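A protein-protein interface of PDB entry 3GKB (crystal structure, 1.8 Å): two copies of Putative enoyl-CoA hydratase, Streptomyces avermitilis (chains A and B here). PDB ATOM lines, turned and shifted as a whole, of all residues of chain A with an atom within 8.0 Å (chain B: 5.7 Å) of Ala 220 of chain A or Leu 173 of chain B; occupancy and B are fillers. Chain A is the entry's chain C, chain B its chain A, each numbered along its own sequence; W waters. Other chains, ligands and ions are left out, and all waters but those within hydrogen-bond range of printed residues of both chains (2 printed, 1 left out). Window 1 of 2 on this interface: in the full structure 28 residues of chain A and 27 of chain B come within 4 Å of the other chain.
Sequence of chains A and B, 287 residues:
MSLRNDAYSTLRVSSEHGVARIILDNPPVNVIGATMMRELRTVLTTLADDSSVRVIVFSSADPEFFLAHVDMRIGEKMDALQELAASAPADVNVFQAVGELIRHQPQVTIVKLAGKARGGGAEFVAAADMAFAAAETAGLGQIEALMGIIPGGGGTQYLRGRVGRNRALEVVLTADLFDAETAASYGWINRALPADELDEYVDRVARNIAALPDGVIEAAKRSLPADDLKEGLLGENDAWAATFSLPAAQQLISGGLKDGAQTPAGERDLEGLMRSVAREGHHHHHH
The backbone carbonyl oxygen (O) of Glu 170 of chain B is in hydrogen-bond range of the side-chain hydroxyl (OG1) of Thr 174 of chain B. The backbone carbonyl oxygen (O) of Thr 174 of chain B lies within hydrogen-bond range of the guanidinium group (NH2) of Arg 275 of chain B, 2.7 Å away. The backbone NH of Val 108 of chain A sits at hydrogen-bond distance from the backbone carbonyl oxygen of Arg 54 of chain A (3.2 Å). The backbone NH of Asp 129 of chain A is in hydrogen-bond range of the side-chain hydroxyl of Thr 109 of chain A (2.9 Å). The backbone carbonyl oxygen (O) of Thr 109 of chain A is in hydrogen-bond range of the backbone NH (N) of Met 130 of chain A (3.1 Å). The backbone carbonyl oxygen (O) of Ala 220 of chain A lies within hydrogen-bond range of the side-chain hydroxyl (OG) of Ser 223 of chain A (2.9 Å).
CD1 of Leu 169 of chain B touches CG of Asp 129 of chain A, at 3.999 Å. CE of Met 130 of chain A touches CA of Glu 170 of chain B, 3.7 Å away. Ile 209 of chain A touches Leu 173 of chain B. Leu 212 of chain A touches Ala 145 of chain B (CD2 to O, 3.6 Å). CD1 of Leu 212 of chain A touches O of Leu 173 of chain B (3.5 Å). Ile 150 of chain B touches Val 216 of chain A (CG2 to O, 3.8 Å). CG2 of Ile 150 of chain B touches CB of Ala 219 of chain A, at 3.8 Å. CD2 of Leu 173 of chain B touches CB of Ala 220 of chain A (3.7 Å). CB of Ala 239 of chain B touches CD of Arg 222 of chain A, 3.9 Å away. Ser 223 of chain A touches Ile 150 of chain B.
Gln 107 of chain A touches none of the printed residues of chain B. Ala 220 of chain A touches just these residues of chain B: Ile 150 and Leu 173. Printed residues of chain A within 4 Å of Ala 145 of chain B: Leu 212, Pro 213 and Val 216. Printed residues of chain A within 4 Å of Leu 169 of chain B: Asp 129 and Leu 224. Leu 173 of chain B touches just these residues of chain A: Val 108 (3.6 Å), Ile 209 (3.6 Å), Leu 212 (3.5 Å) and Ala 220 (3.7 Å). Of the printed residues of chain A, Arg 275 of chain B touches Asn 208. The nearest residue of chain A that does not touch Leu 173 of chain B is Val 216 of chain A (4.1 Å). The nearest printed residue of chain B that does not touch Ala 219 of chain A is Leu 173 of chain B (6.8 Å).
Of the 27 printed residues of chain A, 14 touch a printed residue of chain B. Hydrophobic or aromatic side chains of chain A within 4 Å of the printed part of chain B: Val 108, Met 130, Val 205, Ile 209, Leu 212, Pro 213, Val 216, Ala 219, Ala 220 and Leu 224.
No position is printed for both chains. Of the 18 pairs that touch across the chains among the printed residues, none has its exchanged pair printed and touching as well.
Water W2 bridges the backbone carbonyl oxygen of Asn 208 of chain A (2.7 Å) and the guanidinium group of Arg 275 of chain B (2.8 Å). Water W1 lies within hydrogen-bond range of the side-chain amide nitrogen (ND2) of Asn 208 of chain A (3.0 Å), the backbone carbonyl oxygen (O) of Thr 174 of chain B (3.1 Å) and the guanidinium group (NH2) of Arg 275 of chain B (3.4 Å).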
ATOM      1  N   ARG A  54      11.818 -15.551 -26.556  1.00  0.00           N
ATOM      2  CA  ARG A  54      12.464 -14.260 -26.760  1.00  0.00           C
ATOM      3  C   ARG A  54      13.789 -14.353 -27.544  1.00  0.00           C
ATOM      4  O   ARG A  54      14.209 -13.366 -28.139  1.00  0.00           O
ATOM      5  CB  ARG A  54      12.647 -13.573 -25.399  1.00  0.00           C
ATOM      6  CG  ARG A  54      11.280 -13.085 -24.819  1.00  0.00           C
ATOM      7  CD  ARG A  54      11.343 -12.470 -23.430  1.00  0.00           C
ATOM      8  NE  ARG A  54      12.057 -13.254 -22.412  1.00  0.00           N
ATOM      9  CZ  ARG A  54      11.542 -14.245 -21.686  1.00  0.00           C
ATOM     10  NH1 ARG A  54      10.298 -14.680 -21.884  1.00  0.00           N
ATOM     11  NH2 ARG A  54      12.302 -14.849 -20.786  1.00  0.00           N
ATOM     12  N   VAL A  55      14.428 -15.529 -27.528  1.00  0.00           N
ATOM     13  CA  VAL A  55      15.710 -15.781 -28.170  1.00  0.00           C
ATOM     14  C   VAL A  55      15.654 -17.125 -28.916  1.00  0.00           C
ATOM     15  O   VAL A  55      15.076 -18.074 -28.391  1.00  0.00           O
ATOM     16  CB  VAL A  55      16.848 -15.842 -27.131  1.00  0.00           C
ATOM     17  CG1 VAL A  55      18.153 -16.193 -27.789  1.00  0.00           C
ATOM     18  CG2 VAL A  55      16.895 -14.507 -26.345  1.00  0.00           C
ATOM     19  N   PRO A 106      11.085 -11.814 -35.030  1.00  0.00           N
ATOM     20  CA  PRO A 106      10.955 -10.887 -33.886  1.00  0.00           C
ATOM     21  C   PRO A 106      11.897 -11.217 -32.729  1.00  0.00           C
ATOM     22  O   PRO A 106      12.455 -10.296 -32.089  1.00  0.00           O
ATOM     23  CB  PRO A 106       9.477 -11.013 -33.459  1.00  0.00           C
ATOM     24  CG  PRO A 106       8.880 -12.064 -34.288  1.00  0.00           C
ATOM     25  CD  PRO A 106       9.867 -12.604 -35.278  1.00  0.00           C
ATOM     26  N   GLN A 107      12.104 -12.513 -32.483  1.00  0.00           N
ATOM     27  CA  GLN A 107      13.074 -12.944 -31.490  1.00  0.00           C
ATOM     28  C   GLN A 107      14.485 -12.565 -31.924  1.00  0.00           C
ATOM     29  O   GLN A 107      14.771 -12.422 -33.110  1.00  0.00           O
ATOM     30  CB  GLN A 107      13.050 -14.458 -31.302  1.00  0.00           C
ATOM     31  CG  GLN A 107      11.836 -14.987 -30.552  1.00  0.00           C
ATOM     32  CD  GLN A 107      10.612 -15.224 -31.424  1.00  0.00           C
ATOM     33  OE1 GLN A 107      10.668 -15.097 -32.642  1.00  0.00           O
ATOM     34  NE2 GLN A 107       9.483 -15.556 -30.786  1.00  0.00           N
ATOM     35  N   VAL A 108      15.361 -12.407 -30.939  1.00  0.00           N
ATOM     36  CA  VAL A 108      16.786 -12.345 -31.155  1.00  0.00           C
ATOM     37  C   VAL A 108      17.264 -13.668 -31.727  1.00  0.00           C
ATOM     38  O   VAL A 108      17.027 -14.724 -31.152  1.00  0.00           O
ATOM     39  CB  VAL A 108      17.585 -11.985 -29.875  1.00  0.00           C
ATOM     40  CG1 VAL A 108      19.071 -11.904 -30.207  1.00  0.00           C
ATOM     41  CG2 VAL A 108      17.098 -10.629 -29.294  1.00  0.00           C
ATOM     42  N   THR A 109      17.899 -13.619 -32.884  1.00  0.00           N
ATOM     43  CA  THR A 109      18.401 -14.843 -33.503  1.00  0.00           C
ATOM     44  C   THR A 109      19.926 -14.901 -33.392  1.00  0.00           C
ATOM     45  O   THR A 109      20.647 -13.916 -33.692  1.00  0.00           O
ATOM     46  CB  THR A 109      17.991 -14.978 -34.978  1.00  0.00           C
ATOM     47  OG1 THR A 109      18.425 -13.823 -35.709  1.00  0.00           O
ATOM     48  CG2 THR A 109      16.467 -15.137 -35.134  1.00  0.00           C
ATOM     49  N   ASP A 129      20.752 -12.219 -36.367  1.00  0.00           N
ATOM     50  CA  ASP A 129      21.158 -11.006 -35.630  1.00  0.00           C
ATOM     51  C   ASP A 129      22.635 -11.070 -35.195  1.00  0.00           C
ATOM     52  O   ASP A 129      23.385 -10.081 -35.317  1.00  0.00           O
ATOM     53  CB  ASP A 129      20.275 -10.754 -34.432  1.00  0.00           C
ATOM     54  CG  ASP A 129      18.837 -10.474 -34.814  1.00  0.00           C
ATOM     55  OD1 ASP A 129      18.553 -10.021 -35.963  1.00  0.00           O
ATOM     56  OD2 ASP A 129      17.979 -10.724 -33.952  1.00  0.00           O
ATOM     57  N   MET A 130      23.057 -12.219 -34.677  1.00  0.00           N
ATOM     58  CA  MET A 130      24.440 -12.384 -34.250  1.00  0.00           C
ATOM     59  C   MET A 130      24.919 -13.821 -34.487  1.00  0.00           C
ATOM     60  O   MET A 130      24.130 -14.764 -34.455  1.00  0.00           O
ATOM     61  CB  MET A 130      24.641 -11.926 -32.779  1.00  0.00           C
ATOM     62  CG  MET A 130      23.681 -12.391 -31.760  1.00  0.00           C
ATOM     63  SD  MET A 130      23.701 -11.471 -30.119  1.00  0.00           S
ATOM     64  CE  MET A 130      22.413 -10.245 -30.349  1.00  0.00           C
ATOM     65  N   VAL A 205      25.007 -15.734 -23.356  1.00  0.00           N
ATOM     66  CA  VAL A 205      24.393 -14.634 -24.119  1.00  0.00           C
ATOM     67  C   VAL A 205      22.866 -14.852 -24.271  1.00  0.00           C
ATOM     68  O   VAL A 205      22.066 -13.945 -24.038  1.00  0.00           O
ATOM     69  CB  VAL A 205      25.075 -14.447 -25.501  1.00  0.00           C
ATOM     70  CG1 VAL A 205      24.170 -13.625 -26.446  1.00  0.00           C
ATOM     71  CG2 VAL A 205      26.428 -13.780 -25.333  1.00  0.00           C
ATOM     72  N   ASN A 208      21.140 -14.458 -20.881  1.00  0.00           N
ATOM     73  CA  ASN A 208      21.182 -13.058 -20.474  1.00  0.00           C
ATOM     74  C   ASN A 208      20.178 -12.190 -21.235  1.00  0.00           C
ATOM     75  O   ASN A 208      19.527 -11.334 -20.640  1.00  0.00           O
ATOM     76  CB  ASN A 208      22.607 -12.483 -20.527  1.00  0.00           C
ATOM     77  CG  ASN A 208      23.489 -12.959 -19.358  1.00  0.00           C
ATOM     78  OD1 ASN A 208      23.031 -13.707 -18.466  1.00  0.00           O
ATOM     79  ND2 ASN A 208      24.753 -12.534 -19.359  1.00  0.00           N
ATOM     80  N   ILE A 209      20.061 -12.424 -22.539  1.00  0.00           N
ATOM     81  CA  ILE A 209      19.121 -11.700 -23.370  1.00  0.00           C
ATOM     82  C   ILE A 209      17.683 -12.102 -23.040  1.00  0.00           C
ATOM     83  O   ILE A 209      16.821 -11.225 -22.918  1.00  0.00           O
ATOM     84  CB  ILE A 209      19.444 -11.847 -24.854  1.00  0.00           C
ATOM     85  CG1 ILE A 209      20.788 -11.137 -25.148  1.00  0.00           C
ATOM     86  CG2 ILE A 209      18.304 -11.250 -25.701  1.00  0.00           C
ATOM     87  CD1 ILE A 209      21.356 -11.338 -26.553  1.00  0.00           C
ATOM     88  N   ALA A 210      17.447 -13.411 -22.824  1.00  0.00           N
ATOM     89  CA  ALA A 210      16.120 -13.883 -22.442  1.00  0.00           C
ATOM     90  C   ALA A 210      15.672 -13.325 -21.077  1.00  0.00           C
ATOM     91  O   ALA A 210      14.476 -13.147 -20.872  1.00  0.00           O
ATOM     92  CB  ALA A 210      16.062 -15.422 -22.459  1.00  0.00           C
ATOM     93  N   ALA A 211      16.614 -13.013 -20.179  1.00  0.00           N
ATOM     94  CA  ALA A 211      16.290 -12.465 -18.835  1.00  0.00           C
ATOM     95  C   ALA A 211      15.958 -10.968 -18.852  1.00  0.00           C
ATOM     96  O   ALA A 211      15.434 -10.440 -17.862  1.00  0.00           O
ATOM     97  CB  ALA A 211      17.411 -12.737 -17.845  1.00  0.00           C
ATOM     98  N   LEU A 212      16.219 -10.284 -19.964  1.00  0.00           N
ATOM     99  CA  LEU A 212      15.925  -8.862 -20.053  1.00  0.00           C
ATOM    100  C   LEU A 212      14.442  -8.591 -19.809  1.00  0.00           C
ATOM    101  O   LEU A 212      13.583  -9.375 -20.244  1.00  0.00           O
ATOM    102  CB  LEU A 212      16.318  -8.314 -21.446  1.00  0.00           C
ATOM    103  CG  LEU A 212      17.819  -8.325 -21.666  1.00  0.00           C
ATOM    104  CD1 LEU A 212      18.073  -7.861 -23.086  1.00  0.00           C
ATOM    105  CD2 LEU A 212      18.595  -7.464 -20.662  1.00  0.00           C
ATOM    106  N   PRO A 213      14.118  -7.450 -19.166  1.00  0.00           N
ATOM    107  CA  PRO A 213      12.725  -7.100 -18.902  1.00  0.00           C
ATOM    108  C   PRO A 213      11.846  -7.020 -20.169  1.00  0.00           C
ATOM    109  O   PRO A 213      12.324  -6.820 -21.298  1.00  0.00           O
ATOM    110  CB  PRO A 213      12.834  -5.707 -18.225  1.00  0.00           C
ATOM    111  CG  PRO A 213      14.164  -5.602 -17.764  1.00  0.00           C
ATOM    112  CD  PRO A 213      15.038  -6.437 -18.637  1.00  0.00           C
ATOM    113  N   GLY A 215       9.680  -5.979 -23.159  1.00  0.00           N
ATOM    114  CA  GLY A 215       9.727  -4.875 -24.119  1.00  0.00           C
ATOM    115  C   GLY A 215      11.100  -4.402 -24.576  1.00  0.00           C
ATOM    116  O   GLY A 215      11.202  -3.617 -25.524  1.00  0.00           O
ATOM    117  N   VAL A 216      12.164  -4.823 -23.898  1.00  0.00           N
ATOM    118  CA  VAL A 216      13.501  -4.338 -24.266  1.00  0.00           C
ATOM    119  C   VAL A 216      13.963  -4.842 -25.632  1.00  0.00           C
ATOM    120  O   VAL A 216      14.452  -4.053 -26.445  1.00  0.00           O
ATOM    121  CB  VAL A 216      14.536  -4.655 -23.183  1.00  0.00           C
ATOM    122  CG1 VAL A 216      15.976  -4.258 -23.653  1.00  0.00           C
ATOM    123  CG2 VAL A 216      14.165  -3.926 -21.868  1.00  0.00           C
ATOM    124  N   ILE A 217      13.823  -6.144 -25.878  1.00  0.00           N
ATOM    125  CA  ILE A 217      14.183  -6.710 -27.172  1.00  0.00           C
ATOM    126  C   ILE A 217      13.417  -6.012 -28.276  1.00  0.00           C
ATOM    127  O   ILE A 217      14.000  -5.596 -29.306  1.00  0.00           O
ATOM    128  CB  ILE A 217      13.936  -8.226 -27.241  1.00  0.00           C
ATOM    129  CG1 ILE A 217      14.983  -8.959 -26.393  1.00  0.00           C
ATOM    130  CG2 ILE A 217      14.082  -8.705 -28.700  1.00  0.00           C
ATOM    131  CD1 ILE A 217      14.610 -10.436 -26.052  1.00  0.00           C
ATOM    132  N   GLU A 218      12.116  -5.884 -28.059  1.00  0.00           N
ATOM    133  CA  GLU A 218      11.255  -5.264 -29.046  1.00  0.00           C
ATOM    134  C   GLU A 218      11.682  -3.822 -29.340  1.00  0.00           C
ATOM    135  O   GLU A 218      11.713  -3.398 -30.487  1.00  0.00           O
ATOM    136  CB  GLU A 218       9.795  -5.293 -28.559  1.00  0.00           C
ATOM    137  CG  GLU A 218       9.215  -6.698 -28.447  1.00  0.00           C
ATOM    138  CD  GLU A 218       9.359  -7.386 -27.075  1.00  0.00           C
ATOM    139  OE1 GLU A 218      10.320  -7.147 -26.260  1.00  0.00           O
ATOM    140  OE2 GLU A 218       8.481  -8.260 -26.830  1.00  0.00           O
ATOM    141  N   ALA A 219      12.005  -3.079 -28.293  1.00  0.00           N
ATOM    142  CA  ALA A 219      12.496  -1.705 -28.437  1.00  0.00           C
ATOM    143  C   ALA A 219      13.837  -1.622 -29.201  1.00  0.00           C
ATOM    144  O   ALA A 219      14.021  -0.738 -30.073  1.00  0.00           O
ATOM    145  CB  ALA A 219      12.638  -1.077 -27.062  1.00  0.00           C
ATOM    146  N   ALA A 220      14.750  -2.548 -28.886  1.00  0.00           N
ATOM    147  CA  ALA A 220      16.055  -2.600 -29.551  1.00  0.00           C
ATOM    148  C   ALA A 220      15.869  -2.843 -31.038  1.00  0.00           C
ATOM    149  O   ALA A 220      16.505  -2.186 -31.836  1.00  0.00           O
ATOM    150  CB  ALA A 220      16.977  -3.664 -28.935  1.00  0.00           C
ATOM    151  N   LYS A 221      15.024  -3.809 -31.409  1.00  0.00           N
ATOM    152  CA  LYS A 221      14.772  -4.097 -32.822  1.00  0.00           C
ATOM    153  C   LYS A 221      14.044  -2.969 -33.560  1.00  0.00           C
ATOM    154  O   LYS A 221      14.258  -2.764 -34.750  1.00  0.00           O
ATOM    155  CB  LYS A 221      14.005  -5.410 -32.964  1.00  0.00           C
ATOM    156  CG  LYS A 221      14.882  -6.602 -32.623  1.00  0.00           C
ATOM    157  CD  LYS A 221      14.574  -7.783 -33.537  1.00  0.00           C
ATOM    158  CE  LYS A 221      15.549  -8.874 -33.292  1.00  0.00           C
ATOM    159  NZ  LYS A 221      15.452  -9.889 -34.349  1.00  0.00           N
ATOM    160  N   ARG A 222      13.164  -2.263 -32.850  1.00  0.00           N
ATOM    161  CA  ARG A 222      12.450  -1.104 -33.370  1.00  0.00           C
ATOM    162  C   ARG A 222      13.456   0.012 -33.637  1.00  0.00           C
ATOM    163  O   ARG A 222      13.343   0.697 -34.648  1.00  0.00           O
ATOM    164  CB  ARG A 222      11.329  -0.709 -32.385  1.00  0.00           C
ATOM    165  CG  ARG A 222      10.632   0.667 -32.475  1.00  0.00           C
ATOM    166  CD  ARG A 222       9.591   0.770 -31.298  1.00  0.00           C
ATOM    167  NE  ARG A 222       8.787   1.997 -31.266  1.00  0.00           N
ATOM    168  CZ  ARG A 222       7.960   2.345 -30.269  1.00  0.00           C
ATOM    169  NH1 ARG A 222       7.834   1.595 -29.174  1.00  0.00           N
ATOM    170  NH2 ARG A 222       7.254   3.467 -30.353  1.00  0.00           N
ATOM    171  N   SER A 223      14.473   0.152 -32.780  1.00  0.00           N
ATOM    172  CA  SER A 223      15.455   1.222 -32.936  1.00  0.00           C
ATOM    173  C   SER A 223      16.513   0.903 -33.985  1.00  0.00           C
ATOM    174  O   SER A 223      17.160   1.828 -34.504  1.00  0.00           O
ATOM    175  CB  SER A 223      16.120   1.563 -31.612  1.00  0.00           C
ATOM    176  OG  SER A 223      17.069   0.604 -31.225  1.00  0.00           O
ATOM    177  N   LEU A 224      16.698  -0.400 -34.231  1.00  0.00           N
ATOM    178  CA  LEU A 224      17.674  -0.935 -35.175  1.00  0.00           C
ATOM    179  C   LEU A 224      16.971  -1.847 -36.183  1.00  0.00           C
ATOM    180  O   LEU A 224      17.204  -3.080 -36.216  1.00  0.00           O
ATOM    181  CB  LEU A 224      18.756  -1.700 -34.451  1.00  0.00           C
ATOM    182  CG  LEU A 224      19.652  -0.843 -33.552  1.00  0.00           C
ATOM    183  CD1 LEU A 224      20.293  -1.721 -32.465  1.00  0.00           C
ATOM    184  CD2 LEU A 224      20.693  -0.100 -34.362  1.00  0.00           C
ATOM    185  N   PRO A 225      16.126  -1.247 -37.019  1.00  0.00           N
ATOM    186  CA  PRO A 225      15.357  -2.068 -37.928  1.00  0.00           C
ATOM    187  C   PRO A 225      16.245  -2.726 -38.979  1.00  0.00           C
ATOM    188  O   PRO A 225      17.345  -2.208 -39.312  1.00  0.00           O
ATOM    189  CB  PRO A 225      14.386  -1.072 -38.545  1.00  0.00           C
ATOM    190  CG  PRO A 225      15.082   0.227 -38.439  1.00  0.00           C
ATOM    191  CD  PRO A 225      15.812   0.179 -37.176  1.00  0.00           C
ATOM    192  N   ALA A 226      15.767  -3.859 -39.487  1.00  0.00           N
ATOM    193  CA  ALA A 226      16.434  -4.563 -40.568  1.00  0.00           C
ATOM    194  C   ALA A 226      16.753  -3.639 -41.745  1.00  0.00           C
ATOM    195  O   ALA A 226      15.911  -2.821 -42.134  1.00  0.00           O
ATOM    196  CB  ALA A 226      15.581  -5.756 -41.034  1.00  0.00           C
ATOM    197  N   ALA B 145      19.972  -1.789 -21.203  1.00  0.00           N
ATOM    198  CA  ALA B 145      19.074  -2.989 -21.280  1.00  0.00           C
ATOM    199  C   ALA B 145      18.858  -3.584 -19.898  1.00  0.00           C
ATOM    200  O   ALA B 145      17.748  -4.087 -19.593  1.00  0.00           O
ATOM    201  CB  ALA B 145      19.632  -4.071 -22.215  1.00  0.00           C
ATOM    202  N   ILE B 150      16.510   1.013 -23.406  1.00  0.00           N
ATOM    203  CA  ILE B 150      17.552   0.910 -24.416  1.00  0.00           C
ATOM    204  C   ILE B 150      18.312   2.241 -24.369  1.00  0.00           C
ATOM    205  O   ILE B 150      17.844   3.182 -23.729  1.00  0.00           O
ATOM    206  CB  ILE B 150      16.982   0.641 -25.838  1.00  0.00           C
ATOM    207  CG1 ILE B 150      16.047   1.775 -26.312  1.00  0.00           C
ATOM    208  CG2 ILE B 150      16.273  -0.710 -25.875  1.00  0.00           C
ATOM    209  CD1 ILE B 150      15.850   1.780 -27.797  1.00  0.00           C
ATOM    210  N   ALA B 168      25.689  -3.970 -33.248  1.00  0.00           N
ATOM    211  CA  ALA B 168      24.976  -2.991 -32.432  1.00  0.00           C
ATOM    212  C   ALA B 168      23.929  -3.680 -31.552  1.00  0.00           C
ATOM    213  O   ALA B 168      23.835  -3.404 -30.366  1.00  0.00           O
ATOM    214  CB  ALA B 168      24.335  -1.908 -33.294  1.00  0.00           C
ATOM    215  N   LEU B 169      23.205  -4.646 -32.126  1.00  0.00           N
ATOM    216  CA  LEU B 169      22.248  -5.434 -31.358  1.00  0.00           C
ATOM    217  C   LEU B 169      22.937  -6.258 -30.252  1.00  0.00           C
ATOM    218  O   LEU B 169      22.440  -6.342 -29.142  1.00  0.00           O
ATOM    219  CB  LEU B 169      21.450  -6.383 -32.272  1.00  0.00           C
ATOM    220  CG  LEU B 169      20.314  -5.725 -33.034  1.00  0.00           C
ATOM    221  CD1 LEU B 169      19.788  -6.651 -34.124  1.00  0.00           C
ATOM    222  CD2 LEU B 169      19.223  -5.309 -32.047  1.00  0.00           C
ATOM    223  N   GLU B 170      24.091  -6.840 -30.581  1.00  0.00           N
ATOM    224  CA  GLU B 170      24.908  -7.557 -29.630  1.00  0.00           C
ATOM    225  C   GLU B 170      25.311  -6.641 -28.463  1.00  0.00           C
ATOM    226  O   GLU B 170      25.115  -6.980 -27.314  1.00  0.00           O
ATOM    227  CB  GLU B 170      26.155  -8.130 -30.306  1.00  0.00           C
ATOM    228  CG  GLU B 170      27.035  -8.966 -29.345  1.00  0.00           C
ATOM    229  CD  GLU B 170      28.439  -9.194 -29.859  1.00  0.00           C
ATOM    230  OE1 GLU B 170      28.737  -8.893 -31.040  1.00  0.00           O
ATOM    231  OE2 GLU B 170      29.246  -9.660 -29.036  1.00  0.00           O
ATOM    232  N   VAL B 171      25.839  -5.479 -28.767  1.00  0.00           N
ATOM    233  CA  VAL B 171      26.290  -4.564 -27.687  1.00  0.00           C
ATOM    234  C   VAL B 171      25.117  -4.157 -26.821  1.00  0.00           C
ATOM    235  O   VAL B 171      25.195  -4.210 -25.584  1.00  0.00           O
ATOM    236  CB  VAL B 171      26.976  -3.323 -28.269  1.00  0.00           C
ATOM    237  CG1 VAL B 171      27.188  -2.261 -27.210  1.00  0.00           C
ATOM    238  CG2 VAL B 171      28.310  -3.681 -28.897  1.00  0.00           C
ATOM    239  N   VAL B 172      24.008  -3.801 -27.457  1.00  0.00           N
ATOM    240  CA  VAL B 172      22.831  -3.297 -26.726  1.00  0.00           C
ATOM    241  C   VAL B 172      22.184  -4.383 -25.867  1.00  0.00           C
ATOM    242  O   VAL B 172      21.848  -4.133 -24.708  1.00  0.00           O
ATOM    243  CB  VAL B 172      21.828  -2.614 -27.677  1.00  0.00           C
ATOM    244  CG1 VAL B 172      20.402  -2.385 -27.011  1.00  0.00           C
ATOM    245  CG2 VAL B 172      22.456  -1.323 -28.183  1.00  0.00           C
ATOM    246  N   LEU B 173      22.029  -5.597 -26.415  1.00  0.00           N
ATOM    247  CA  LEU B 173      21.216  -6.607 -25.721  1.00  0.00           C
ATOM    248  C   LEU B 173      22.048  -7.477 -24.775  1.00  0.00           C
ATOM    249  O   LEU B 173      21.522  -7.899 -23.736  1.00  0.00           O
ATOM    250  CB  LEU B 173      20.433  -7.465 -26.696  1.00  0.00           C
ATOM    251  CG  LEU B 173      19.369  -6.685 -27.457  1.00  0.00           C
ATOM    252  CD1 LEU B 173      18.829  -7.569 -28.582  1.00  0.00           C
ATOM    253  CD2 LEU B 173      18.265  -6.117 -26.544  1.00  0.00           C
ATOM    254  N   THR B 174      23.316  -7.747 -25.100  1.00  0.00           N
ATOM    255  CA  THR B 174      24.196  -8.441 -24.143  1.00  0.00           C
ATOM    256  C   THR B 174      24.489  -7.515 -22.961  1.00  0.00           C
ATOM    257  O   THR B 174      24.702  -7.984 -21.864  1.00  0.00           O
ATOM    258  CB  THR B 174      25.536  -8.957 -24.749  1.00  0.00           C
ATOM    259  OG1 THR B 174      26.394  -7.843 -25.119  1.00  0.00           O
ATOM    260  CG2 THR B 174      25.277  -9.906 -25.946  1.00  0.00           C
ATOM    261  N   ALA B 175      24.513  -6.198 -23.201  1.00  0.00           N
ATOM    262  CA  ALA B 175      24.840  -5.211 -22.154  1.00  0.00           C
ATOM    263  C   ALA B 175      26.163  -5.479 -21.446  1.00  0.00           C
ATOM    264  O   ALA B 175      26.378  -5.016 -20.319  1.00  0.00           O
ATOM    265  CB  ALA B 175      23.706  -5.084 -21.117  1.00  0.00           C
ATOM    266  N   ALA B 239      11.304   4.435 -29.115  1.00  0.00           N
ATOM    267  CA  ALA B 239      11.553   3.113 -28.514  1.00  0.00           C
ATOM    268  C   ALA B 239      11.943   3.224 -27.033  1.00  0.00           C
ATOM    269  O   ALA B 239      11.470   2.451 -26.181  1.00  0.00           O
ATOM    270  CB  ALA B 239      12.609   2.317 -29.357  1.00  0.00           C
ATOM    271  N   ARG B 275      22.035  -7.259 -12.989  1.00  0.00           N
ATOM    272  CA  ARG B 275      21.427  -8.580 -13.182  1.00  0.00           C
ATOM    273  C   ARG B 275      20.915  -9.181 -11.856  1.00  0.00           C
ATOM    274  O   ARG B 275      19.875  -9.856 -11.846  1.00  0.00           O
ATOM    275  CB  ARG B 275      22.363  -9.549 -13.881  1.00  0.00           C
ATOM    276  CG  ARG B 275      22.480  -9.229 -15.373  1.00  0.00           C
ATOM    277  CD  ARG B 275      23.124 -10.314 -16.162  1.00  0.00           C
ATOM    278  NE  ARG B 275      23.106  -9.921 -17.558  1.00  0.00           N
ATOM    279  CZ  ARG B 275      24.126  -9.383 -18.207  1.00  0.00           C
ATOM    280  NH1 ARG B 275      25.317  -9.219 -17.633  1.00  0.00           N
ATOM    281  NH2 ARG B 275      23.959  -9.025 -19.453  1.00  0.00           N
HETATM  282  O   HOH W   1      25.392 -10.975 -21.843  1.00  0.00           O
HETATM  283  O   HOH W   2      20.439 -10.132 -18.341  1.00  0.00           O
